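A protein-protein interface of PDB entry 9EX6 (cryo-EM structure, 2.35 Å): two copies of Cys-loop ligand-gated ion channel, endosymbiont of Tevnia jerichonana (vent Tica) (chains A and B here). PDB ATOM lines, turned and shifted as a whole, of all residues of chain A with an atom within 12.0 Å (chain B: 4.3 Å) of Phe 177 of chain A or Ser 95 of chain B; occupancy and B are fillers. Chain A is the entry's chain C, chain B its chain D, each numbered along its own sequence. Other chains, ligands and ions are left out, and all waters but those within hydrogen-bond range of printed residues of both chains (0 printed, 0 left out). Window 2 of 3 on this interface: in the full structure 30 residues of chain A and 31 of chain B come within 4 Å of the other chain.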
ATOM      1  N   ARG A  74     -20.849  12.572  -8.714  1.00  0.00           N
ATOM      2  CA  ARG A  74     -19.517  13.077  -8.378  1.00  0.00           C
ATOM      3  C   ARG A  74     -18.495  11.943  -8.268  1.00  0.00           C
ATOM      4  O   ARG A  74     -18.740  10.935  -7.597  1.00  0.00           O
ATOM      5  CB  ARG A  74     -19.554  13.881  -7.076  1.00  0.00           C
ATOM      6  CG  ARG A  74     -18.251  14.618  -6.754  1.00  0.00           C
ATOM      7  CD  ARG A  74     -18.309  15.447  -5.466  1.00  0.00           C
ATOM      8  NE  ARG A  74     -19.461  16.339  -5.419  1.00  0.00           N
ATOM      9  CZ  ARG A  74     -19.583  17.460  -6.116  1.00  0.00           C
ATOM     10  NH1 ARG A  74     -18.585  17.936  -6.843  1.00  0.00           N
ATOM     11  NH2 ARG A  74     -20.698  18.174  -6.004  1.00  0.00           N
ATOM     12  N   THR A  79      -4.798  13.619  -6.979  1.00  0.00           N
ATOM     13  CA  THR A  79      -3.626  14.179  -7.660  1.00  0.00           C
ATOM     14  C   THR A  79      -2.320  13.722  -7.001  1.00  0.00           C
ATOM     15  O   THR A  79      -2.277  13.441  -5.801  1.00  0.00           O
ATOM     16  CB  THR A  79      -3.680  15.718  -7.696  1.00  0.00           C
ATOM     17  OG1 THR A  79      -2.605  16.211  -8.505  1.00  0.00           O
ATOM     18  CG2 THR A  79      -3.570  16.309  -6.296  1.00  0.00           C
ATOM     19  N   HIS A  81       1.209  14.560  -5.643  1.00  0.00           N
ATOM     20  CA  HIS A  81       1.641  15.874  -5.173  1.00  0.00           C
ATOM     21  C   HIS A  81       3.138  16.163  -5.361  1.00  0.00           C
ATOM     22  O   HIS A  81       3.453  17.344  -5.537  1.00  0.00           O
ATOM     23  CB  HIS A  81       1.212  16.080  -3.719  1.00  0.00           C
ATOM     24  CG  HIS A  81       1.649  17.394  -3.125  1.00  0.00           C
ATOM     25  ND1 HIS A  81       0.996  18.576  -3.398  1.00  0.00           N
ATOM     26  CD2 HIS A  81       2.648  17.709  -2.260  1.00  0.00           C
ATOM     27  CE1 HIS A  81       1.574  19.562  -2.732  1.00  0.00           C
ATOM     28  NE2 HIS A  81       2.582  19.065  -2.039  1.00  0.00           N
ATOM     29  N   ASP A 134      -2.998  12.759  -3.127  1.00  0.00           N
ATOM     30  CA  ASP A 134      -3.885  13.673  -2.407  1.00  0.00           C
ATOM     31  C   ASP A 134      -5.303  13.677  -2.974  1.00  0.00           C
ATOM     32  O   ASP A 134      -5.496  13.754  -4.188  1.00  0.00           O
ATOM     33  CB  ASP A 134      -3.360  15.110  -2.449  1.00  0.00           C
ATOM     34  CG  ASP A 134      -2.127  15.316  -1.600  1.00  0.00           C
ATOM     35  OD1 ASP A 134      -1.753  14.400  -0.838  1.00  0.00           O
ATOM     36  OD2 ASP A 134      -1.536  16.413  -1.689  1.00  0.00           O
ATOM     37  N   SER A 135      -6.289  13.646  -2.076  1.00  0.00           N
ATOM     38  CA  SER A 135      -7.689  13.812  -2.451  1.00  0.00           C
ATOM     39  C   SER A 135      -8.002  15.281  -2.717  1.00  0.00           C
ATOM     40  O   SER A 135      -7.513  16.172  -2.019  1.00  0.00           O
ATOM     41  CB  SER A 135      -8.605  13.280  -1.345  1.00  0.00           C
ATOM     42  OG  SER A 135      -9.966  13.601  -1.593  1.00  0.00           O
ATOM     43  N   ILE A 136      -8.829  15.537  -3.726  1.00  0.00           N
ATOM     44  CA  ILE A 136      -9.159  16.921  -4.057  1.00  0.00           C
ATOM     45  C   ILE A 136     -10.315  17.430  -3.205  1.00  0.00           C
ATOM     46  O   ILE A 136     -10.290  18.574  -2.745  1.00  0.00           O
ATOM     47  CB  ILE A 136      -9.484  17.047  -5.560  1.00  0.00           C
ATOM     48  CG1 ILE A 136      -8.231  16.887  -6.425  1.00  0.00           C
ATOM     49  CG2 ILE A 136     -10.152  18.378  -5.863  1.00  0.00           C
ATOM     50  CD1 ILE A 136      -8.509  16.958  -7.914  1.00  0.00           C
ATOM     51  N   PHE A 137     -11.313  16.607  -2.949  1.00  0.00           N
ATOM     52  CA  PHE A 137     -12.480  16.993  -2.181  1.00  0.00           C
ATOM     53  C   PHE A 137     -12.217  16.842  -0.684  1.00  0.00           C
ATOM     54  O   PHE A 137     -11.311  16.114  -0.273  1.00  0.00           O
ATOM     55  CB  PHE A 137     -13.676  16.131  -2.620  1.00  0.00           C
ATOM     56  CG  PHE A 137     -14.244  16.542  -3.962  1.00  0.00           C
ATOM     57  CD1 PHE A 137     -14.894  17.767  -4.090  1.00  0.00           C
ATOM     58  CD2 PHE A 137     -14.077  15.762  -5.087  1.00  0.00           C
ATOM     59  CE1 PHE A 137     -15.383  18.201  -5.304  1.00  0.00           C
ATOM     60  CE2 PHE A 137     -14.585  16.183  -6.313  1.00  0.00           C
ATOM     61  CZ  PHE A 137     -15.241  17.420  -6.412  1.00  0.00           C
ATOM     62  N   PRO A 138     -12.958  17.536   0.174  1.00  0.00           N
ATOM     63  CA  PRO A 138     -12.643  17.494   1.603  1.00  0.00           C
ATOM     64  C   PRO A 138     -13.291  16.288   2.275  1.00  0.00           C
ATOM     65  O   PRO A 138     -14.165  15.623   1.722  1.00  0.00           O
ATOM     66  CB  PRO A 138     -13.231  18.810   2.122  1.00  0.00           C
ATOM     67  CG  PRO A 138     -14.406  19.025   1.236  1.00  0.00           C
ATOM     68  CD  PRO A 138     -13.960  18.568  -0.134  1.00  0.00           C
ATOM     69  N   HIS A 140     -15.290  15.264   4.424  1.00  0.00           N
ATOM     70  CA  HIS A 140     -16.674  14.936   4.742  1.00  0.00           C
ATOM     71  C   HIS A 140     -17.461  14.483   3.525  1.00  0.00           C
ATOM     72  O   HIS A 140     -18.565  13.956   3.687  1.00  0.00           O
ATOM     73  CB  HIS A 140     -17.386  16.112   5.433  1.00  0.00           C
ATOM     74  CG  HIS A 140     -17.403  17.391   4.647  1.00  0.00           C
ATOM     75  ND1 HIS A 140     -18.415  17.698   3.765  1.00  0.00           N
ATOM     76  CD2 HIS A 140     -16.565  18.458   4.645  1.00  0.00           C
ATOM     77  CE1 HIS A 140     -18.184  18.884   3.228  1.00  0.00           C
ATOM     78  NE2 HIS A 140     -17.072  19.368   3.748  1.00  0.00           N
ATOM     79  N   LEU A 141     -16.910  14.657   2.327  1.00  0.00           N
ATOM     80  CA  LEU A 141     -17.445  14.027   1.131  1.00  0.00           C
ATOM     81  C   LEU A 141     -16.872  12.622   0.934  1.00  0.00           C
ATOM     82  O   LEU A 141     -17.631  11.656   0.812  1.00  0.00           O
ATOM     83  CB  LEU A 141     -17.166  14.921  -0.080  1.00  0.00           C
ATOM     84  CG  LEU A 141     -18.056  16.170  -0.180  1.00  0.00           C
ATOM     85  CD1 LEU A 141     -17.445  17.170  -1.169  1.00  0.00           C
ATOM     86  CD2 LEU A 141     -19.510  15.903  -0.473  1.00  0.00           C
ATOM     87  N   THR A 173      -3.426  13.742   6.381  1.00  0.00           N
ATOM     88  CA  THR A 173      -4.315  14.755   5.806  1.00  0.00           C
ATOM     89  C   THR A 173      -3.536  15.955   5.268  1.00  0.00           C
ATOM     90  O   THR A 173      -2.375  16.179   5.615  1.00  0.00           O
ATOM     91  CB  THR A 173      -5.348  15.276   6.818  1.00  0.00           C
ATOM     92  OG1 THR A 173      -4.680  15.619   8.034  1.00  0.00           O
ATOM     93  CG2 THR A 173      -6.404  14.217   7.106  1.00  0.00           C
ATOM     94  N   HIS A 174      -4.205  16.742   4.415  1.00  0.00           N
ATOM     95  CA  HIS A 174      -3.665  17.983   3.862  1.00  0.00           C
ATOM     96  C   HIS A 174      -4.797  19.000   3.753  1.00  0.00           C
ATOM     97  O   HIS A 174      -5.976  18.655   3.866  1.00  0.00           O
ATOM     98  CB  HIS A 174      -3.004  17.763   2.490  1.00  0.00           C
ATOM     99  CG  HIS A 174      -3.981  17.585   1.366  1.00  0.00           C
ATOM    100  ND1 HIS A 174      -4.309  18.608   0.507  1.00  0.00           N
ATOM    101  CD2 HIS A 174      -4.704  16.509   0.967  1.00  0.00           C
ATOM    102  CE1 HIS A 174      -5.192  18.173  -0.376  1.00  0.00           C
ATOM    103  NE2 HIS A 174      -5.448  16.904  -0.119  1.00  0.00           N
ATOM    104  N   ASN A 175      -4.440  20.269   3.518  1.00  0.00           N
ATOM    105  CA  ASN A 175      -5.410  21.360   3.560  1.00  0.00           C
ATOM    106  C   ASN A 175      -5.120  22.406   2.488  1.00  0.00           C
ATOM    107  O   ASN A 175      -3.965  22.781   2.275  1.00  0.00           O
ATOM    108  CB  ASN A 175      -5.415  22.033   4.942  1.00  0.00           C
ATOM    109  CG  ASN A 175      -6.617  22.928   5.153  1.00  0.00           C
ATOM    110  OD1 ASN A 175      -6.696  24.021   4.589  1.00  0.00           O
ATOM    111  ND2 ASN A 175      -7.540  22.489   6.008  1.00  0.00           N
ATOM    112  N   GLU A 176      -6.181  22.884   1.823  1.00  0.00           N
ATOM    113  CA  GLU A 176      -6.089  23.967   0.845  1.00  0.00           C
ATOM    114  C   GLU A 176      -7.255  24.940   1.022  1.00  0.00           C
ATOM    115  O   GLU A 176      -8.379  24.513   1.281  1.00  0.00           O
ATOM    116  CB  GLU A 176      -6.094  23.439  -0.603  1.00  0.00           C
ATOM    117  CG  GLU A 176      -4.807  22.748  -1.046  1.00  0.00           C
ATOM    118  CD  GLU A 176      -3.635  23.702  -1.212  1.00  0.00           C
ATOM    119  OE1 GLU A 176      -3.825  24.925  -1.065  1.00  0.00           O
ATOM    120  OE2 GLU A 176      -2.521  23.220  -1.505  1.00  0.00           O
ATOM    121  N   PHE A 177      -6.989  26.213   0.705  1.00  0.00           N
ATOM    122  CA  PHE A 177      -8.008  27.283   0.796  1.00  0.00           C
ATOM    123  C   PHE A 177      -8.517  27.465   2.221  1.00  0.00           C
ATOM    124  O   PHE A 177      -9.644  27.932   2.409  1.00  0.00           O
ATOM    125  CB  PHE A 177      -9.160  27.091  -0.222  1.00  0.00           C
ATOM    126  CG  PHE A 177      -8.702  26.977  -1.654  1.00  0.00           C
ATOM    127  CD1 PHE A 177      -7.819  27.897  -2.199  1.00  0.00           C
ATOM    128  CD2 PHE A 177      -9.161  25.945  -2.457  1.00  0.00           C
ATOM    129  CE1 PHE A 177      -7.405  27.792  -3.515  1.00  0.00           C
ATOM    130  CE2 PHE A 177      -8.749  25.834  -3.774  1.00  0.00           C
ATOM    131  CZ  PHE A 177      -7.871  26.759  -4.304  1.00  0.00           C
ATOM    132  N   THR A 178      -7.688  27.117   3.211  1.00  0.00           N
ATOM    133  CA  THR A 178      -8.052  27.262   4.633  1.00  0.00           C
ATOM    134  C   THR A 178      -9.490  26.840   4.921  1.00  0.00           C
ATOM    135  O   THR A 178     -10.249  27.577   5.561  1.00  0.00           O
ATOM    136  CB  THR A 178      -7.797  28.703   5.137  1.00  0.00           C
ATOM    137  N   LYS A 179      -9.864  25.651   4.458  1.00  0.00           N
ATOM    138  CA  LYS A 179     -11.229  25.186   4.642  1.00  0.00           C
ATOM    139  C   LYS A 179     -11.226  23.798   5.258  1.00  0.00           C
ATOM    140  O   LYS A 179     -10.822  23.636   6.412  1.00  0.00           O
ATOM    141  CB  LYS A 179     -11.979  25.203   3.304  1.00  0.00           C
ATOM    142  N   GLY A 180     -11.659  22.800   4.497  1.00  0.00           N
ATOM    143  CA  GLY A 180     -11.736  21.451   5.021  1.00  0.00           C
ATOM    144  C   GLY A 180     -10.516  20.596   4.802  1.00  0.00           C
ATOM    145  O   GLY A 180      -9.901  20.644   3.735  1.00  0.00           O
ATOM    146  N   ASP A 181     -10.151  19.808   5.809  1.00  0.00           N
ATOM    147  CA  ASP A 181      -9.042  18.872   5.666  1.00  0.00           C
ATOM    148  C   ASP A 181      -9.394  17.792   4.645  1.00  0.00           C
ATOM    149  O   ASP A 181     -10.561  17.424   4.497  1.00  0.00           O
ATOM    150  CB  ASP A 181      -8.683  18.212   6.997  1.00  0.00           C
ATOM    151  CG  ASP A 181      -7.983  19.153   7.977  1.00  0.00           C
ATOM    152  OD1 ASP A 181      -7.428  20.194   7.559  1.00  0.00           O
ATOM    153  OD2 ASP A 181      -7.897  18.783   9.163  1.00  0.00           O
ATOM    154  N   ALA A 182      -8.379  17.272   3.950  1.00  0.00           N
ATOM    155  CA  ALA A 182      -8.585  16.225   2.951  1.00  0.00           C
ATOM    156  C   ALA A 182      -7.534  15.130   3.110  1.00  0.00           C
ATOM    157  O   ALA A 182      -6.424  15.380   3.577  1.00  0.00           O
ATOM    158  CB  ALA A 182      -8.547  16.788   1.520  1.00  0.00           C
ATOM    159  N   ARG A 184      -4.684  12.176   2.566  1.00  0.00           N
ATOM    160  CA  ARG A 184      -3.406  11.972   1.885  1.00  0.00           C
ATOM    161  C   ARG A 184      -2.936  10.538   2.104  1.00  0.00           C
ATOM    162  O   ARG A 184      -2.979  10.040   3.233  1.00  0.00           O
ATOM    163  CB  ARG A 184      -2.338  12.957   2.392  1.00  0.00           C
ATOM    164  CG  ARG A 184      -0.936  12.661   1.873  1.00  0.00           C
ATOM    165  CD  ARG A 184       0.041  13.799   2.166  1.00  0.00           C
ATOM    166  NE  ARG A 184      -0.038  14.862   1.169  1.00  0.00           N
ATOM    167  CZ  ARG A 184       0.608  16.015   1.262  1.00  0.00           C
ATOM    168  NH1 ARG A 184       1.366  16.303   2.305  1.00  0.00           N
ATOM    169  NH2 ARG A 184       0.456  16.919   0.299  1.00  0.00           N
ATOM    170  N   ARG B  37      -1.058  31.550  -6.785  1.00  0.00           N
ATOM    171  CA  ARG B  37      -2.372  31.717  -6.156  1.00  0.00           C
ATOM    172  C   ARG B  37      -2.990  33.092  -6.381  1.00  0.00           C
ATOM    173  O   ARG B  37      -2.296  34.103  -6.283  1.00  0.00           O
ATOM    174  CB  ARG B  37      -2.258  31.453  -4.656  1.00  0.00           C
ATOM    175  CG  ARG B  37      -2.370  29.986  -4.276  1.00  0.00           C
ATOM    176  CD  ARG B  37      -3.776  29.619  -3.842  1.00  0.00           C
ATOM    177  NE  ARG B  37      -4.243  30.468  -2.752  1.00  0.00           N
ATOM    178  CZ  ARG B  37      -5.324  31.239  -2.809  1.00  0.00           C
ATOM    179  NH1 ARG B  37      -6.070  31.281  -3.906  1.00  0.00           N
ATOM    180  NH2 ARG B  37      -5.651  31.976  -1.758  1.00  0.00           N
ATOM    181  N   ARG B  57     -18.590  25.768  -4.281  1.00  0.00           N
ATOM    182  CA  ARG B  57     -18.582  25.076  -5.563  1.00  0.00           C
ATOM    183  C   ARG B  57     -17.153  24.972  -6.095  1.00  0.00           C
ATOM    184  O   ARG B  57     -16.304  25.822  -5.807  1.00  0.00           O
ATOM    185  CB  ARG B  57     -19.507  25.803  -6.548  1.00  0.00           C
ATOM    186  CG  ARG B  57     -20.986  25.394  -6.389  1.00  0.00           C
ATOM    187  CD  ARG B  57     -22.018  26.315  -7.077  1.00  0.00           C
ATOM    188  NE  ARG B  57     -23.381  25.916  -6.722  1.00  0.00           N
ATOM    189  CZ  ARG B  57     -24.484  26.351  -7.318  1.00  0.00           C
ATOM    190  NH1 ARG B  57     -24.448  27.291  -8.244  1.00  0.00           N
ATOM    191  NH2 ARG B  57     -25.664  25.889  -6.910  1.00  0.00           N
ATOM    192  N   LEU B  93      -6.977  24.410 -10.266  1.00  0.00           N
ATOM    193  CA  LEU B  93      -8.174  24.185  -9.457  1.00  0.00           C
ATOM    194  C   LEU B  93      -8.809  25.498  -9.010  1.00  0.00           C
ATOM    195  O   LEU B  93      -8.103  26.453  -8.686  1.00  0.00           O
ATOM    196  CB  LEU B  93      -7.825  23.337  -8.223  1.00  0.00           C
ATOM    197  CG  LEU B  93      -8.870  23.028  -7.146  1.00  0.00           C
ATOM    198  CD1 LEU B  93      -9.988  22.154  -7.685  1.00  0.00           C
ATOM    199  CD2 LEU B  93      -8.203  22.353  -5.971  1.00  0.00           C
ATOM    200  N   ILE B  94     -10.144  25.516  -8.926  1.00  0.00           N
ATOM    201  CA  ILE B  94     -10.923  26.717  -8.633  1.00  0.00           C
ATOM    202  C   ILE B  94     -11.962  26.421  -7.555  1.00  0.00           C
ATOM    203  O   ILE B  94     -12.694  25.429  -7.646  1.00  0.00           O
ATOM    204  CB  ILE B  94     -11.603  27.294  -9.890  1.00  0.00           C
ATOM    205  CG1 ILE B  94     -10.580  28.118 -10.668  1.00  0.00           C
ATOM    206  CG2 ILE B  94     -12.764  28.171  -9.472  1.00  0.00           C
ATOM    207  CD1 ILE B  94     -11.106  28.707 -11.941  1.00  0.00           C
ATOM    208  N   SER B  95     -12.007  27.280  -6.527  1.00  0.00           N
ATOM    209  CA  SER B  95     -13.082  27.314  -5.534  1.00  0.00           C
ATOM    210  C   SER B  95     -13.910  28.590  -5.666  1.00  0.00           C
ATOM    211  O   SER B  95     -13.350  29.685  -5.765  1.00  0.00           O
ATOM    212  CB  SER B  95     -12.510  27.250  -4.121  1.00  0.00           C
ATOM    213  OG  SER B  95     -13.510  27.065  -3.142  1.00  0.00           O
ATOM    214  N   LEU B  96     -15.238  28.456  -5.595  1.00  0.00           N
ATOM    215  CA  LEU B  96     -16.170  29.566  -5.783  1.00  0.00           C
ATOM    216  C   LEU B  96     -17.047  29.720  -4.547  1.00  0.00           C
ATOM    217  O   LEU B  96     -17.732  28.773  -4.143  1.00  0.00           O
ATOM    218  CB  LEU B  96     -17.038  29.354  -7.024  1.00  0.00           C
ATOM    219  CG  LEU B  96     -18.076  30.446  -7.303  1.00  0.00           C
ATOM    220  CD1 LEU B  96     -17.413  31.791  -7.559  1.00  0.00           C
ATOM    221  CD2 LEU B  96     -18.978  30.054  -8.457  1.00  0.00           C
ATOM    222  N   SER B  97     -17.037  30.918  -3.971  1.00  0.00           N
ATOM    223  CA  SER B  97     -17.731  31.225  -2.731  1.00  0.00           C
ATOM    224  C   SER B  97     -19.177  31.654  -2.974  1.00  0.00           C
ATOM    225  O   SER B  97     -19.535  32.160  -4.042  1.00  0.00           O
ATOM    226  CB  SER B  97     -16.999  32.333  -1.971  1.00  0.00           C
ATOM    227  OG  SER B  97     -17.791  32.781  -0.887  1.00  0.00           O
ATOM    228  N   THR B 101     -16.741  35.224  -4.337  1.00  0.00           N
ATOM    229  CA  THR B 101     -15.288  35.251  -4.247  1.00  0.00           C
ATOM    230  C   THR B 101     -14.711  34.061  -5.000  1.00  0.00           C
ATOM    231  O   THR B 101     -15.135  32.922  -4.785  1.00  0.00           O
ATOM    232  CB  THR B 101     -14.831  35.218  -2.790  1.00  0.00           C
ATOM    233  OG1 THR B 101     -15.426  36.303  -2.070  1.00  0.00           O
ATOM    234  CG2 THR B 101     -13.318  35.339  -2.713  1.00  0.00           C
ATOM    235  N   VAL B 102     -13.739  34.324  -5.872  1.00  0.00           N
ATOM    236  CA  VAL B 102     -13.065  33.276  -6.631  1.00  0.00           C
ATOM    237  C   VAL B 102     -11.681  33.049  -6.039  1.00  0.00           C
ATOM    238  O   VAL B 102     -10.919  34.002  -5.837  1.00  0.00           O
ATOM    239  CB  VAL B 102     -12.954  33.639  -8.122  1.00  0.00           C
ATOM    240  CG1 VAL B 102     -12.344  32.475  -8.887  1.00  0.00           C
ATOM    241  CG2 VAL B 102     -14.313  33.997  -8.693  1.00  0.00           C
ATOM    242  N   MET B 103     -11.350  31.786  -5.773  1.00  0.00           N
ATOM    243  CA  MET B 103     -10.015  31.390  -5.348  1.00  0.00           C
ATOM    244  C   MET B 103      -9.427  30.442  -6.386  1.00  0.00           C
ATOM    245  O   MET B 103     -10.040  29.421  -6.712  1.00  0.00           O
ATOM    246  CB  MET B 103     -10.039  30.734  -3.963  1.00  0.00           C
ATOM    247  CG  MET B 103     -10.617  31.619  -2.861  1.00  0.00           C
ATOM    248  SD  MET B 103     -10.598  30.865  -1.221  1.00  0.00           S
ATOM    249  CE  MET B 103      -8.888  31.089  -0.748  1.00  0.00           C
ATOM    250  N   LEU B 105      -5.848  28.349  -8.062  1.00  0.00           N
ATOM    251  CA  LEU B 105      -4.560  27.739  -7.749  1.00  0.00           C
ATOM    252  C   LEU B 105      -4.054  26.950  -8.950  1.00  0.00           C
ATOM    253  O   LEU B 105      -4.817  26.190  -9.552  1.00  0.00           O
ATOM    254  CB  LEU B 105      -4.693  26.817  -6.526  1.00  0.00           C
ATOM    255  CG  LEU B 105      -3.594  25.773  -6.301  1.00  0.00           C
ATOM    256  CD1 LEU B 105      -2.270  26.386  -5.873  1.00  0.00           C
ATOM    257  CD2 LEU B 105      -3.984  24.590  -5.401  1.00  0.00           C
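The backbone carbonyl oxygen (O) of Leu 105 of chain B sits at hydrogen-bond distance from the backbone NH (N) of Leu 93 of chain B (2.9 Å).
N of Met 103 of chain B lies within hydrogen-bond range of O of Ser 95 of chain B, 2.9 Å away.
CE1 of Phe 177 of chain A touches NH1 of Arg 37 of chain B (3.8 Å).
Phe 177 of chain A touches Ser 95 of chain B (CD2 to CB, 3.96 Å).
CD1 of Phe 177 of chain A touches CE of Met 103 of chain B, at 3.7 Å.
Leu 105 of chain B touches Phe 177 of chain A.
Asn 175 of chain A touches none of the printed residues of chain B.
Of chain B, only Arg 37, Ser 95, Met 103 and Leu 105 come within 4 Å of Phe 177 of chain A.
Arg 184 of chain A touches none of the printed residues of chain B.
Of the printed residues of chain A, Arg 37 of chain B touches Phe 177.
Of chain A, only Phe 177 (3.96 Å) comes within 4 Å of Ser 95 of chain B.
No residue of chain A comes within 4 Å of Leu 96 of chain B.
No residue of chain A comes within 4 Å of Ser 97 of chain B.
Thr 101 of chain B touches none of the printed residues of chain A.
No residue of chain A comes within 4 Å of Val 102 of chain B.
Of chain A, only Phe 177 (3.7 Å) comes within 4 Å of Met 103 of chain B.
Printed residues of chain A within 4 Å of Leu 105 of chain B: Phe 177.
The nearest residue of chain A that does not touch Ser 95 of chain B is Lys 179 of chain A (6.9 Å).
The nearest printed residue of chain A that does not touch Arg 37 of chain B is Glu 176 of chain A (5.5 Å).
Of the 21 printed residues of chain A, 1 touches a printed residue of chain B.
Hydrophobic or aromatic side chains of chain A that line the printed part of chain B: Phe 177.
Of the 11 printed residues of chain B, 4 touch a printed residue of chain A.
Printed residues of chain B that touch a printed residue of chain A: Arg 37, Ser 95, Met 103 and Leu 105.
Among the printed residues, 4 pairs touch across the chains.
No position is printed for both chains.
Of the 4 pairs that touch across the chains among the printed residues, none has its exchanged pair printed and touching as well.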
